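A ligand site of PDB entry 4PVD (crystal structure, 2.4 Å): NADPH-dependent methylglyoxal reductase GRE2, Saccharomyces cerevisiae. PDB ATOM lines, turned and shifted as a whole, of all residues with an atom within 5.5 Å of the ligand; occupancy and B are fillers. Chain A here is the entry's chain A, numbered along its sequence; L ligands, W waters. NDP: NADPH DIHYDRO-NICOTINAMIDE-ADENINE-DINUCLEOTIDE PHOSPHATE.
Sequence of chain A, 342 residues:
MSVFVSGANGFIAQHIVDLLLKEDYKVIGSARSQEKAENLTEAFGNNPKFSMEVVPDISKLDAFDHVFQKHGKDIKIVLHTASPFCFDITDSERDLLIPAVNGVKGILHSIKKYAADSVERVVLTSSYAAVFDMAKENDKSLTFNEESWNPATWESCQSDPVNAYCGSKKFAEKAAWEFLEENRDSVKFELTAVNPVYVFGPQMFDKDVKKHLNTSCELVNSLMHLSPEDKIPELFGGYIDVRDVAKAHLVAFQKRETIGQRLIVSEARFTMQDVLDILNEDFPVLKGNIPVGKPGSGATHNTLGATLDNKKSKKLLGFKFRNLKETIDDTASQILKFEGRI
OD1 of Asp 57 lies within hydrogen-bond range of OG of Ser 59, 2.7 Å away.
OG of Ser 126 sits at hydrogen-bond distance from ND2 of Asn 195, at 3.2 Å.
The side-chain hydroxyl of Ser 216 lies within hydrogen-bond range of the side-chain amide nitrogen of Asn 214 (3.0 Å).
The backbone carbonyl oxygen (O) of Pro 196 lies within hydrogen-bond range of the backbone NH (N) of Tyr 128, 2.9 Å away.
The backbone carbonyl oxygen (O) of Val 199 lies within hydrogen-bond range of the side-chain hydroxyl (OG) of Ser 216, 2.7 Å away.
The backbone carbonyl oxygen (O) of Thr 125 sits at hydrogen-bond distance from the side-chain amino group (NZ) of Lys 169 (2.9 Å).
The backbone carbonyl oxygen of Ser 127 lies within hydrogen-bond range of the side-chain amide nitrogen of Asn 195 (3.0 Å).
Water W2 lies within hydrogen-bond range of ND2 of Asn 214 (2.9 Å), O2N of the ligand (3.1 Å) and N of Ser 216 (3.1 Å).
Water W1 bridges OH of Tyr 165 and OG of Ser 127.
Water W3 lies within hydrogen-bond range of OG1 of Thr 81 (2.5 Å) and O of Gly 7 (2.7 Å).
The side-chain amino group of Lys 36 lies within salt-bridge range of an oxygen (O2X) of the ligand.
An oxygen (O1N) of the ligand lies within hydrogen-bond range of the backbone NH (N) of Ile 12, 3.0 Å away.
O3D of the ligand sits at hydrogen-bond distance from O of Thr 81 (2.7 Å).
An oxygen (O1X) of the ligand lies within salt-bridge range of the guanidinium group (NH2) of Arg 32, at 3.5 Å.
N6A of the ligand is in hydrogen-bond range of OD2 of Asp 57.
OG of Ser 216 sits at hydrogen-bond distance from N7N of the ligand (3.0 Å).
The backbone carbonyl oxygen (O) of Gly 7 sits at hydrogen-bond distance from an oxygen (O3B) of the ligand (3.5 Å).
The backbone NH of Val 199 lies within hydrogen-bond range of an oxygen (O7N) of the ligand, 2.8 Å away.
The side-chain hydroxyl (OH) of Tyr 165 lies within hydrogen-bond range of an oxygen (O2D) of the ligand (3.0 Å).
O1A of the ligand is in hydrogen-bond range of N of Phe 11 (3.0 Å).
A nitrogen (N1A) of the ligand sits at hydrogen-bond distance from the backbone NH of Ile 58, 3.0 Å away.
O3B of the ligand is in hydrogen-bond range of OD1 of Asn 9, 3.0 Å away.
An oxygen (O3B) of the ligand lies within hydrogen-bond range of the backbone NH (N) of Gly 10, at 3.5 Å.
O2D of the ligand is in hydrogen-bond range of NZ of Lys 169 (2.7 Å).
Pro 56 touches the ligand.
CA of Ala 82 touches O4B of the ligand, 3.7 Å away.
CB of Ser 83 touches O3D of the ligand, 3.1 Å away.
Pro 84 touches the ligand.
Phe 85 touches the ligand.
Thr 125 touches the ligand (CG2 to O4D, 3.3 Å).
Ser 126 touches the ligand (O to C6N, 3.2 Å).
Ser 127 touches the ligand (OG to C5N, 3.4 Å).
O of Pro 196 touches C5N of the ligand (3.3 Å).
Val 197 touches the ligand.
Tyr 198 touches the ligand (CA to O7N, 3.5 Å).
CB of Asn 214 touches O1A of the ligand, at 3.98 Å.
Hydrophobic or aromatic side chains that line the ligand: Phe 11, Ile 12, Ile 58, Ala 82, Pro 84, Phe 85, Tyr 165, Pro 196 and Val 199.
Of the 33 residues printed, 26 come within 4 Å of the ligand.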
ATOM      1  N   GLY A   7     -36.066  12.482  -7.126  1.00  0.00           N
ATOM      2  CA  GLY A   7     -35.237  12.740  -8.313  1.00  0.00           C
ATOM      3  C   GLY A   7     -35.735  12.018  -9.541  1.00  0.00           C
ATOM      4  O   GLY A   7     -34.969  11.342 -10.226  1.00  0.00           O
ATOM      5  N   ALA A   8     -37.029  12.173  -9.827  1.00  0.00           N
ATOM      6  CA  ALA A   8     -37.734  11.351 -10.831  1.00  0.00           C
ATOM      7  C   ALA A   8     -37.312  11.632 -12.277  1.00  0.00           C
ATOM      8  O   ALA A   8     -37.549  10.813 -13.161  1.00  0.00           O
ATOM      9  CB  ALA A   8     -39.242  11.523 -10.673  1.00  0.00           C
ATOM     10  N   ASN A   9     -36.704  12.795 -12.505  1.00  0.00           N
ATOM     11  CA  ASN A   9     -36.243  13.181 -13.837  1.00  0.00           C
ATOM     12  C   ASN A   9     -34.827  12.713 -14.125  1.00  0.00           C
ATOM     13  O   ASN A   9     -34.295  12.997 -15.214  1.00  0.00           O
ATOM     14  CB  ASN A   9     -36.267  14.702 -13.959  1.00  0.00           C
ATOM     15  CG  ASN A   9     -35.199  15.350 -13.104  1.00  0.00           C
ATOM     16  OD1 ASN A   9     -35.145  15.127 -11.895  1.00  0.00           O
ATOM     17  ND2 ASN A   9     -34.348  16.147 -13.733  1.00  0.00           N
ATOM     18  N   GLY A  10     -34.200  12.043 -13.167  1.00  0.00           N
ATOM     19  CA  GLY A  10     -32.859  11.516 -13.346  1.00  0.00           C
ATOM     20  C   GLY A  10     -32.794  10.370 -14.345  1.00  0.00           C
ATOM     21  O   GLY A  10     -33.830   9.802 -14.734  1.00  0.00           O
ATOM     22  N   PHE A  11     -31.580  10.019 -14.752  1.00  0.00           N
ATOM     23  CA  PHE A  11     -31.368   9.016 -15.807  1.00  0.00           C
ATOM     24  C   PHE A  11     -31.965   7.646 -15.442  1.00  0.00           C
ATOM     25  O   PHE A  11     -32.779   7.098 -16.182  1.00  0.00           O
ATOM     26  CB  PHE A  11     -29.868   8.934 -16.150  1.00  0.00           C
ATOM     27  CG  PHE A  11     -29.488   7.706 -16.946  1.00  0.00           C
ATOM     28  CD1 PHE A  11     -30.029   7.474 -18.209  1.00  0.00           C
ATOM     29  CD2 PHE A  11     -28.560   6.797 -16.439  1.00  0.00           C
ATOM     30  CE1 PHE A  11     -29.668   6.350 -18.947  1.00  0.00           C
ATOM     31  CE2 PHE A  11     -28.187   5.671 -17.170  1.00  0.00           C
ATOM     32  CZ  PHE A  11     -28.743   5.448 -18.435  1.00  0.00           C
ATOM     33  N   ILE A  12     -31.549   7.119 -14.305  1.00  0.00           N
ATOM     34  CA  ILE A  12     -32.080   5.853 -13.776  1.00  0.00           C
ATOM     35  C   ILE A  12     -33.571   5.964 -13.454  1.00  0.00           C
ATOM     36  O   ILE A  12     -34.389   5.170 -13.919  1.00  0.00           O
ATOM     37  CB  ILE A  12     -31.275   5.404 -12.531  1.00  0.00           C
ATOM     38  CG1 ILE A  12     -29.810   5.129 -12.933  1.00  0.00           C
ATOM     39  CG2 ILE A  12     -31.930   4.204 -11.860  1.00  0.00           C
ATOM     40  CD1 ILE A  12     -28.884   4.756 -11.801  1.00  0.00           C
ATOM     41  N   ALA A  13     -33.893   6.989 -12.668  1.00  0.00           N
ATOM     42  CA  ALA A  13     -35.248   7.226 -12.153  1.00  0.00           C
ATOM     43  C   ALA A  13     -36.338   7.296 -13.201  1.00  0.00           C
ATOM     44  O   ALA A  13     -37.438   6.801 -12.953  1.00  0.00           O
ATOM     45  CB  ALA A  13     -35.275   8.492 -11.311  1.00  0.00           C
ATOM     46  N   ARG A  32     -36.492  19.195  -9.118  1.00  0.00           N
ATOM     47  CA  ARG A  32     -35.960  20.406  -8.500  1.00  0.00           C
ATOM     48  C   ARG A  32     -36.744  21.664  -8.824  1.00  0.00           C
ATOM     49  O   ARG A  32     -36.633  22.668  -8.127  1.00  0.00           O
ATOM     50  CB  ARG A  32     -34.477  20.567  -8.821  1.00  0.00           C
ATOM     51  CG  ARG A  32     -33.610  19.569  -8.069  1.00  0.00           C
ATOM     52  CD  ARG A  32     -32.353  20.214  -7.545  1.00  0.00           C
ATOM     53  NE  ARG A  32     -31.168  19.978  -8.358  1.00  0.00           N
ATOM     54  CZ  ARG A  32     -29.918  20.206  -7.955  1.00  0.00           C
ATOM     55  NH1 ARG A  32     -29.677  20.679  -6.740  1.00  0.00           N
ATOM     56  NH2 ARG A  32     -28.899  19.955  -8.775  1.00  0.00           N
ATOM     57  N   LYS A  36     -38.996  21.306 -14.667  1.00  0.00           N
ATOM     58  CA  LYS A  36     -38.562  19.918 -14.861  1.00  0.00           C
ATOM     59  C   LYS A  36     -39.679  18.930 -14.559  1.00  0.00           C
ATOM     60  O   LYS A  36     -39.762  17.866 -15.179  1.00  0.00           O
ATOM     61  CB  LYS A  36     -37.335  19.610 -13.991  1.00  0.00           C
ATOM     62  CG  LYS A  36     -36.042  20.245 -14.470  1.00  0.00           C
ATOM     63  CD  LYS A  36     -34.997  20.200 -13.367  1.00  0.00           C
ATOM     64  CE  LYS A  36     -33.605  20.530 -13.909  1.00  0.00           C
ATOM     65  NZ  LYS A  36     -32.609  20.720 -12.803  1.00  0.00           N
ATOM     66  N   VAL A  55     -39.232  19.561  -5.172  1.00  0.00           N
ATOM     67  CA  VAL A  55     -38.327  19.505  -4.019  1.00  0.00           C
ATOM     68  C   VAL A  55     -36.958  20.019  -4.475  1.00  0.00           C
ATOM     69  O   VAL A  55     -36.142  19.250  -4.992  1.00  0.00           O
ATOM     70  CB  VAL A  55     -38.211  18.069  -3.447  1.00  0.00           C
ATOM     71  CG1 VAL A  55     -37.072  17.974  -2.417  1.00  0.00           C
ATOM     72  CG2 VAL A  55     -39.542  17.615  -2.832  1.00  0.00           C
ATOM     73  N   PRO A  56     -36.696  21.331  -4.282  1.00  0.00           N
ATOM     74  CA  PRO A  56     -35.534  21.951  -4.948  1.00  0.00           C
ATOM     75  C   PRO A  56     -34.148  21.488  -4.492  1.00  0.00           C
ATOM     76  O   PRO A  56     -33.216  21.532  -5.284  1.00  0.00           O
ATOM     77  CB  PRO A  56     -35.709  23.455  -4.643  1.00  0.00           C
ATOM     78  CG  PRO A  56     -37.116  23.607  -4.188  1.00  0.00           C
ATOM     79  CD  PRO A  56     -37.486  22.317  -3.530  1.00  0.00           C
ATOM     80  N   ASP A  57     -34.008  21.061  -3.229  1.00  0.00           N
ATOM     81  CA  ASP A  57     -32.687  20.757  -2.667  1.00  0.00           C
ATOM     82  C   ASP A  57     -32.769  19.723  -1.552  1.00  0.00           C
ATOM     83  O   ASP A  57     -33.395  19.976  -0.514  1.00  0.00           O
ATOM     84  CB  ASP A  57     -32.029  22.033  -2.146  1.00  0.00           C
ATOM     85  CG  ASP A  57     -30.593  21.827  -1.681  1.00  0.00           C
ATOM     86  OD1 ASP A  57     -30.081  22.719  -0.974  1.00  0.00           O
ATOM     87  OD2 ASP A  57     -29.957  20.798  -2.021  1.00  0.00           O
ATOM     88  N   ILE A  58     -32.134  18.583  -1.753  1.00  0.00           N
ATOM     89  CA  ILE A  58     -32.141  17.515  -0.755  1.00  0.00           C
ATOM     90  C   ILE A  58     -31.119  17.725   0.367  1.00  0.00           C
ATOM     91  O   ILE A  58     -31.068  16.935   1.311  1.00  0.00           O
ATOM     92  CB  ILE A  58     -32.021  16.099  -1.403  1.00  0.00           C
ATOM     93  CG1 ILE A  58     -30.663  15.919  -2.103  1.00  0.00           C
ATOM     94  CG2 ILE A  58     -33.190  15.839  -2.351  1.00  0.00           C
ATOM     95  CD1 ILE A  58     -30.446  14.526  -2.657  1.00  0.00           C
ATOM     96  N   SER A  59     -30.308  18.776   0.286  1.00  0.00           N
ATOM     97  CA  SER A  59     -29.390  19.095   1.374  1.00  0.00           C
ATOM     98  C   SER A  59     -30.158  19.658   2.576  1.00  0.00           C
ATOM     99  O   SER A  59     -29.657  19.658   3.709  1.00  0.00           O
ATOM    100  CB  SER A  59     -28.281  20.057   0.912  1.00  0.00           C
ATOM    101  OG  SER A  59     -28.676  21.419   0.980  1.00  0.00           O
ATOM    102  N   THR A  81     -33.911   7.890  -4.818  1.00  0.00           N
ATOM    103  CA  THR A  81     -32.873   7.777  -5.826  1.00  0.00           C
ATOM    104  C   THR A  81     -32.031   9.054  -5.984  1.00  0.00           C
ATOM    105  O   THR A  81     -30.938   9.015  -6.525  1.00  0.00           O
ATOM    106  CB  THR A  81     -33.450   7.365  -7.203  1.00  0.00           C
ATOM    107  OG1 THR A  81     -33.873   8.543  -7.898  1.00  0.00           O
ATOM    108  CG2 THR A  81     -34.633   6.396  -7.062  1.00  0.00           C
ATOM    109  N   ALA A  82     -32.544  10.177  -5.479  1.00  0.00           N
ATOM    110  CA  ALA A  82     -31.850  11.453  -5.639  1.00  0.00           C
ATOM    111  C   ALA A  82     -30.549  11.525  -4.837  1.00  0.00           C
ATOM    112  O   ALA A  82     -30.544  11.229  -3.633  1.00  0.00           O
ATOM    113  CB  ALA A  82     -32.764  12.611  -5.303  1.00  0.00           C
ATOM    114  N   SER A  83     -29.456  11.881  -5.512  1.00  0.00           N
ATOM    115  CA  SER A  83     -28.154  12.088  -4.882  1.00  0.00           C
ATOM    116  C   SER A  83     -27.262  12.802  -5.892  1.00  0.00           C
ATOM    117  O   SER A  83     -27.329  12.511  -7.087  1.00  0.00           O
ATOM    118  CB  SER A  83     -27.517  10.755  -4.472  1.00  0.00           C
ATOM    119  OG  SER A  83     -26.712  10.902  -3.308  1.00  0.00           O
ATOM    120  N   PRO A  84     -26.434  13.752  -5.432  1.00  0.00           N
ATOM    121  CA  PRO A  84     -25.581  14.434  -6.412  1.00  0.00           C
ATOM    122  C   PRO A  84     -24.548  13.491  -7.044  1.00  0.00           C
ATOM    123  O   PRO A  84     -23.816  12.811  -6.333  1.00  0.00           O
ATOM    124  CB  PRO A  84     -24.892  15.528  -5.587  1.00  0.00           C
ATOM    125  CG  PRO A  84     -25.030  15.093  -4.169  1.00  0.00           C
ATOM    126  CD  PRO A  84     -26.330  14.352  -4.094  1.00  0.00           C
ATOM    127  N   PHE A  85     -24.528  13.458  -8.375  1.00  0.00           N
ATOM    128  CA  PHE A  85     -23.565  12.648  -9.133  1.00  0.00           C
ATOM    129  C   PHE A  85     -23.022  13.543 -10.249  1.00  0.00           C
ATOM    130  O   PHE A  85     -23.025  13.194 -11.427  1.00  0.00           O
ATOM    131  CB  PHE A  85     -24.245  11.371  -9.660  1.00  0.00           C
ATOM    132  CG  PHE A  85     -23.298  10.390 -10.324  1.00  0.00           C
ATOM    133  CD1 PHE A  85     -21.925  10.424 -10.080  1.00  0.00           C
ATOM    134  CD2 PHE A  85     -23.808   9.416 -11.181  1.00  0.00           C
ATOM    135  CE1 PHE A  85     -21.068   9.505 -10.690  1.00  0.00           C
ATOM    136  CE2 PHE A  85     -22.962   8.491 -11.803  1.00  0.00           C
ATOM    137  CZ  PHE A  85     -21.600   8.530 -11.552  1.00  0.00           C
ATOM    138  N   PRO A  99     -25.289  16.986   0.973  1.00  0.00           N
ATOM    139  CA  PRO A  99     -26.557  16.756   0.282  1.00  0.00           C
ATOM    140  C   PRO A  99     -26.974  15.282   0.207  1.00  0.00           C
ATOM    141  O   PRO A  99     -28.141  14.966   0.406  1.00  0.00           O
ATOM    142  CB  PRO A  99     -26.299  17.306  -1.128  1.00  0.00           C
ATOM    143  CG  PRO A  99     -25.211  18.314  -0.934  1.00  0.00           C
ATOM    144  CD  PRO A  99     -24.326  17.690   0.093  1.00  0.00           C
ATOM    145  N   THR A 125     -31.292   3.961  -3.612  1.00  0.00           N
ATOM    146  CA  THR A 125     -30.296   3.861  -4.672  1.00  0.00           C
ATOM    147  C   THR A 125     -28.965   4.259  -4.054  1.00  0.00           C
ATOM    148  O   THR A 125     -28.672   5.444  -3.864  1.00  0.00           O
ATOM    149  CB  THR A 125     -30.597   4.780  -5.859  1.00  0.00           C
ATOM    150  OG1 THR A 125     -31.968   4.631  -6.260  1.00  0.00           O
ATOM    151  CG2 THR A 125     -29.683   4.421  -7.028  1.00  0.00           C
ATOM    152  N   SER A 126     -28.189   3.250  -3.695  1.00  0.00           N
ATOM    153  CA  SER A 126     -26.842   3.471  -3.193  1.00  0.00           C
ATOM    154  C   SER A 126     -25.927   3.252  -4.399  1.00  0.00           C
ATOM    155  O   SER A 126     -26.289   3.627  -5.514  1.00  0.00           O
ATOM    156  CB  SER A 126     -26.542   2.515  -2.041  1.00  0.00           C
ATOM    157  OG  SER A 126     -25.198   2.662  -1.596  1.00  0.00           O
ATOM    158  N   SER A 127     -24.752   2.653  -4.167  1.00  0.00           N
ATOM    159  CA  SER A 127     -23.792   2.406  -5.246  1.00  0.00           C
ATOM    160  C   SER A 127     -22.808   1.275  -4.919  1.00  0.00           C
ATOM    161  O   SER A 127     -22.566   0.958  -3.754  1.00  0.00           O
ATOM    162  CB  SER A 127     -23.033   3.689  -5.569  1.00  0.00           C
ATOM    163  OG  SER A 127     -22.120   3.520  -6.633  1.00  0.00           O
ATOM    164  N   TYR A 128     -22.235   0.679  -5.969  1.00  0.00           N
ATOM    165  CA  TYR A 128     -21.071  -0.192  -5.818  1.00  0.00           C
ATOM    166  C   TYR A 128     -19.882   0.604  -5.250  1.00  0.00           C
ATOM    167  O   TYR A 128     -18.965   0.027  -4.668  1.00  0.00           O
ATOM    168  CB  TYR A 128     -20.688  -0.823  -7.158  1.00  0.00           C
ATOM    169  CG  TYR A 128     -19.486  -1.733  -7.080  1.00  0.00           C
ATOM    170  CD1 TYR A 128     -19.494  -2.849  -6.246  1.00  0.00           C
ATOM    171  CD2 TYR A 128     -18.354  -1.488  -7.848  1.00  0.00           C
ATOM    172  CE1 TYR A 128     -18.399  -3.698  -6.169  1.00  0.00           C
ATOM    173  CE2 TYR A 128     -17.240  -2.331  -7.773  1.00  0.00           C
ATOM    174  CZ  TYR A 128     -17.274  -3.433  -6.934  1.00  0.00           C
ATOM    175  OH  TYR A 128     -16.183  -4.269  -6.860  1.00  0.00           O
ATOM    176  N   TYR A 165     -17.313  11.566  -3.792  1.00  0.00           N
ATOM    177  CA  TYR A 165     -18.542  10.992  -4.319  1.00  0.00           C
ATOM    178  C   TYR A 165     -18.765   9.564  -3.817  1.00  0.00           C
ATOM    179  O   TYR A 165     -19.876   9.212  -3.403  1.00  0.00           O
ATOM    180  CB  TYR A 165     -18.598  11.029  -5.850  1.00  0.00           C
ATOM    181  CG  TYR A 165     -19.715  10.160  -6.375  1.00  0.00           C
ATOM    182  CD1 TYR A 165     -21.041  10.583  -6.290  1.00  0.00           C
ATOM    183  CD2 TYR A 165     -19.452   8.892  -6.892  1.00  0.00           C
ATOM    184  CE1 TYR A 165     -22.082   9.765  -6.735  1.00  0.00           C
ATOM    185  CE2 TYR A 165     -20.483   8.077  -7.338  1.00  0.00           C
ATOM    186  CZ  TYR A 165     -21.795   8.519  -7.257  1.00  0.00           C
ATOM    187  OH  TYR A 165     -22.812   7.695  -7.701  1.00  0.00           O
ATOM    188  N   LYS A 169     -21.837   8.234  -1.182  1.00  0.00           N
ATOM    189  CA  LYS A 169     -22.679   7.047  -1.347  1.00  0.00           C
ATOM    190  C   LYS A 169     -22.591   6.145  -0.105  1.00  0.00           C
ATOM    191  O   LYS A 169     -23.620   5.752   0.452  1.00  0.00           O
ATOM    192  CB  LYS A 169     -22.354   6.290  -2.637  1.00  0.00           C
ATOM    193  CG  LYS A 169     -22.552   7.125  -3.933  1.00  0.00           C
ATOM    194  CD  LYS A 169     -23.959   7.752  -4.062  1.00  0.00           C
ATOM    195  CE  LYS A 169     -25.040   6.694  -4.253  1.00  0.00           C
ATOM    196  NZ  LYS A 169     -26.429   7.266  -4.384  1.00  0.00           N
ATOM    197  N   ASN A 195     -27.418  -1.310  -5.266  1.00  0.00           N
ATOM    198  CA  ASN A 195     -26.052  -0.794  -5.441  1.00  0.00           C
ATOM    199  C   ASN A 195     -25.477  -1.007  -6.839  1.00  0.00           C
ATOM    200  O   ASN A 195     -24.693  -1.935  -7.054  1.00  0.00           O
ATOM    201  CB  ASN A 195     -25.106  -1.441  -4.411  1.00  0.00           C
ATOM    202  CG  ASN A 195     -25.535  -1.176  -2.978  1.00  0.00           C
ATOM    203  OD1 ASN A 195     -26.591  -1.648  -2.534  1.00  0.00           O
ATOM    204  ND2 ASN A 195     -24.697  -0.449  -2.233  1.00  0.00           N
ATOM    205  N   PRO A 196     -25.832  -0.136  -7.783  1.00  0.00           N
ATOM    206  CA  PRO A 196     -25.374  -0.340  -9.151  1.00  0.00           C
ATOM    207  C   PRO A 196     -23.906  -0.044  -9.384  1.00  0.00           C
ATOM    208  O   PRO A 196     -23.291   0.763  -8.677  1.00  0.00           O
ATOM    209  CB  PRO A 196     -26.231   0.645  -9.951  1.00  0.00           C
ATOM    210  CG  PRO A 196     -27.372   0.999  -9.040  1.00  0.00           C
ATOM    211  CD  PRO A 196     -26.763   0.995  -7.701  1.00  0.00           C
ATOM    212  N   VAL A 197     -23.342  -0.723 -10.374  1.00  0.00           N
ATOM    213  CA  VAL A 197     -22.028  -0.411 -10.901  1.00  0.00           C
ATOM    214  C   VAL A 197     -22.245   0.684 -11.933  1.00  0.00           C
ATOM    215  O   VAL A 197     -23.271   1.367 -11.891  1.00  0.00           O
ATOM    216  CB  VAL A 197     -21.372  -1.656 -11.551  1.00  0.00           C
ATOM    217  CG1 VAL A 197     -20.766  -2.542 -10.489  1.00  0.00           C
ATOM    218  CG2 VAL A 197     -22.382  -2.429 -12.368  1.00  0.00           C
ATOM    219  N   TYR A 198     -21.302   0.874 -12.857  1.00  0.00           N
ATOM    220  CA  TYR A 198     -21.483   1.853 -13.923  1.00  0.00           C
ATOM    221  C   TYR A 198     -22.718   1.522 -14.724  1.00  0.00           C
ATOM    222  O   TYR A 198     -22.845   0.404 -15.230  1.00  0.00           O
ATOM    223  CB  TYR A 198     -20.287   1.890 -14.852  1.00  0.00           C
ATOM    224  CG  TYR A 198     -19.082   2.450 -14.192  1.00  0.00           C
ATOM    225  CD1 TYR A 198     -18.867   3.824 -14.140  1.00  0.00           C
ATOM    226  CD2 TYR A 198     -18.129   1.607 -13.628  1.00  0.00           C
ATOM    227  CE1 TYR A 198     -17.749   4.343 -13.527  1.00  0.00           C
ATOM    228  CE2 TYR A 198     -17.008   2.119 -13.020  1.00  0.00           C
ATOM    229  CZ  TYR A 198     -16.824   3.488 -12.973  1.00  0.00           C
ATOM    230  OH  TYR A 198     -15.704   3.999 -12.366  1.00  0.00           O
ATOM    231  N   VAL A 199     -23.607   2.498 -14.849  1.00  0.00           N
ATOM    232  CA  VAL A 199     -24.893   2.299 -15.502  1.00  0.00           C
ATOM    233  C   VAL A 199     -24.869   2.889 -16.899  1.00  0.00           C
ATOM    234  O   VAL A 199     -24.585   4.082 -17.078  1.00  0.00           O
ATOM    235  CB  VAL A 199     -26.047   2.888 -14.662  1.00  0.00           C
ATOM    236  CG1 VAL A 199     -27.403   2.565 -15.273  1.00  0.00           C
ATOM    237  CG2 VAL A 199     -26.009   2.339 -13.247  1.00  0.00           C
ATOM    238  N   ASN A 214     -25.668  12.487 -18.593  1.00  0.00           N
ATOM    239  CA  ASN A 214     -25.422  12.100 -17.205  1.00  0.00           C
ATOM    240  C   ASN A 214     -24.053  11.439 -17.147  1.00  0.00           C
ATOM    241  O   ASN A 214     -23.663  10.731 -18.075  1.00  0.00           O
ATOM    242  CB  ASN A 214     -26.491  11.117 -16.732  1.00  0.00           C
ATOM    243  CG  ASN A 214     -26.559   9.875 -17.590  1.00  0.00           C
ATOM    244  OD1 ASN A 214     -27.118   9.898 -18.690  1.00  0.00           O
ATOM    245  ND2 ASN A 214     -25.987   8.785 -17.106  1.00  0.00           N
ATOM    246  N   SER A 216     -22.313   8.865 -15.943  1.00  0.00           N
ATOM    247  CA  SER A 216     -22.067   7.469 -16.338  1.00  0.00           C
ATOM    248  C   SER A 216     -22.173   7.254 -17.851  1.00  0.00           C
ATOM    249  O   SER A 216     -21.336   6.583 -18.446  1.00  0.00           O
ATOM    250  CB  SER A 216     -22.973   6.499 -15.592  1.00  0.00           C
ATOM    251  OG  SER A 216     -24.300   6.533 -16.076  1.00  0.00           O
HETATM  252  PA  NDP L   1     -28.487  11.721 -12.716  1.00  0.00           P
HETATM  253  O1A NDP L   1     -29.284  11.744 -13.960  1.00  0.00           O
HETATM  254  O2A NDP L   1     -27.586  12.900 -12.625  1.00  0.00           O
HETATM  255  O5B NDP L   1     -29.470  11.661 -11.443  1.00  0.00           O
HETATM  256  C5B NDP L   1     -29.313  12.505 -10.324  1.00  0.00           C
HETATM  257  C4B NDP L   1     -30.683  12.916  -9.794  1.00  0.00           C
HETATM  258  O4B NDP L   1     -30.566  13.439  -8.483  1.00  0.00           O
HETATM  259  C3B NDP L   1     -31.293  14.035 -10.637  1.00  0.00           C
HETATM  260  O3B NDP L   1     -32.695  13.903 -10.664  1.00  0.00           O
HETATM  261  C2B NDP L   1     -30.902  15.271  -9.860  1.00  0.00           C
HETATM  262  O2B NDP L   1     -31.683  16.407 -10.152  1.00  0.00           O
HETATM  263  C1B NDP L   1     -31.045  14.758  -8.440  1.00  0.00           C
HETATM  264  N9A NDP L   1     -30.262  15.578  -7.510  1.00  0.00           N
HETATM  265  C8A NDP L   1     -28.893  15.642  -7.417  1.00  0.00           C
HETATM  266  N7A NDP L   1     -28.594  16.525  -6.440  1.00  0.00           N
HETATM  267  C5A NDP L   1     -29.745  17.007  -5.911  1.00  0.00           C
HETATM  268  C6A NDP L   1     -30.028  17.923  -4.901  1.00  0.00           C
HETATM  269  N6A NDP L   1     -29.048  18.399  -4.136  1.00  0.00           N
HETATM  270  N1A NDP L   1     -31.330  18.222  -4.595  1.00  0.00           N
HETATM  271  C2A NDP L   1     -32.373  17.617  -5.273  1.00  0.00           C
HETATM  272  N3A NDP L   1     -32.093  16.710  -6.277  1.00  0.00           N
HETATM  273  C4A NDP L   1     -30.804  16.421  -6.584  1.00  0.00           C
HETATM  274  O3  NDP L   1     -27.621  10.376 -12.594  1.00  0.00           O
HETATM  275  PN  NDP L   1     -28.161   8.912 -12.197  1.00  0.00           P
HETATM  276  O1N NDP L   1     -29.565   8.720 -12.638  1.00  0.00           O
HETATM  277  O2N NDP L   1     -27.104   7.983 -12.644  1.00  0.00           O
HETATM  278  O5D NDP L   1     -28.105   8.897 -10.591  1.00  0.00           O
HETATM  279  C5D NDP L   1     -29.255   8.682  -9.800  1.00  0.00           C
HETATM  280  C4D NDP L   1     -28.865   7.857  -8.570  1.00  0.00           C
HETATM  281  O4D NDP L   1     -28.225   6.669  -8.985  1.00  0.00           O
HETATM  282  C3D NDP L   1     -27.874   8.611  -7.698  1.00  0.00           C
HETATM  283  O3D NDP L   1     -28.261   8.446  -6.350  1.00  0.00           O
HETATM  284  C2D NDP L   1     -26.537   7.937  -7.991  1.00  0.00           C
HETATM  285  O2D NDP L   1     -25.665   7.927  -6.897  1.00  0.00           O
HETATM  286  C1D NDP L   1     -27.001   6.529  -8.302  1.00  0.00           C
HETATM  287  N1N NDP L   1     -25.997   5.759  -9.049  1.00  0.00           N
HETATM  288  C2N NDP L   1     -25.726   5.984 -10.384  1.00  0.00           C
HETATM  289  C3N NDP L   1     -24.832   5.176 -11.083  1.00  0.00           C
HETATM  290  C7N NDP L   1     -24.519   5.399 -12.542  1.00  0.00           C
HETATM  291  O7N NDP L   1     -23.439   4.677 -13.113  1.00  0.00           O
HETATM  292  N7N NDP L   1     -25.255   6.245 -13.259  1.00  0.00           N
HETATM  293  C4N NDP L   1     -24.130   4.020 -10.401  1.00  0.00           C
HETATM  294  C5N NDP L   1     -24.512   3.867  -8.962  1.00  0.00           C
HETATM  295  C6N NDP L   1     -25.416   4.738  -8.355  1.00  0.00           C
HETATM  296  P2B NDP L   1     -31.350  17.260 -11.484  1.00  0.00           P
HETATM  297  O1X NDP L   1     -29.975  17.879 -11.341  1.00  0.00           O
HETATM  298  O2X NDP L   1     -32.377  18.342 -11.669  1.00  0.00           O
HETATM  299  O3X NDP L   1     -31.385  16.370 -12.706  1.00  0.00           O
HETATM  300  O   HOH W   1     -21.558   5.403  -8.593  1.00  0.00           O
HETATM  301  O   HOH W   2     -24.990   9.423 -14.432  1.00  0.00           O
HETATM  302  O   HOH W   3     -32.720  10.293  -9.213  1.00  0.00           O
HETATM  303  O   HOH W   4     -32.101   8.959 -11.528  1.00  0.00           O
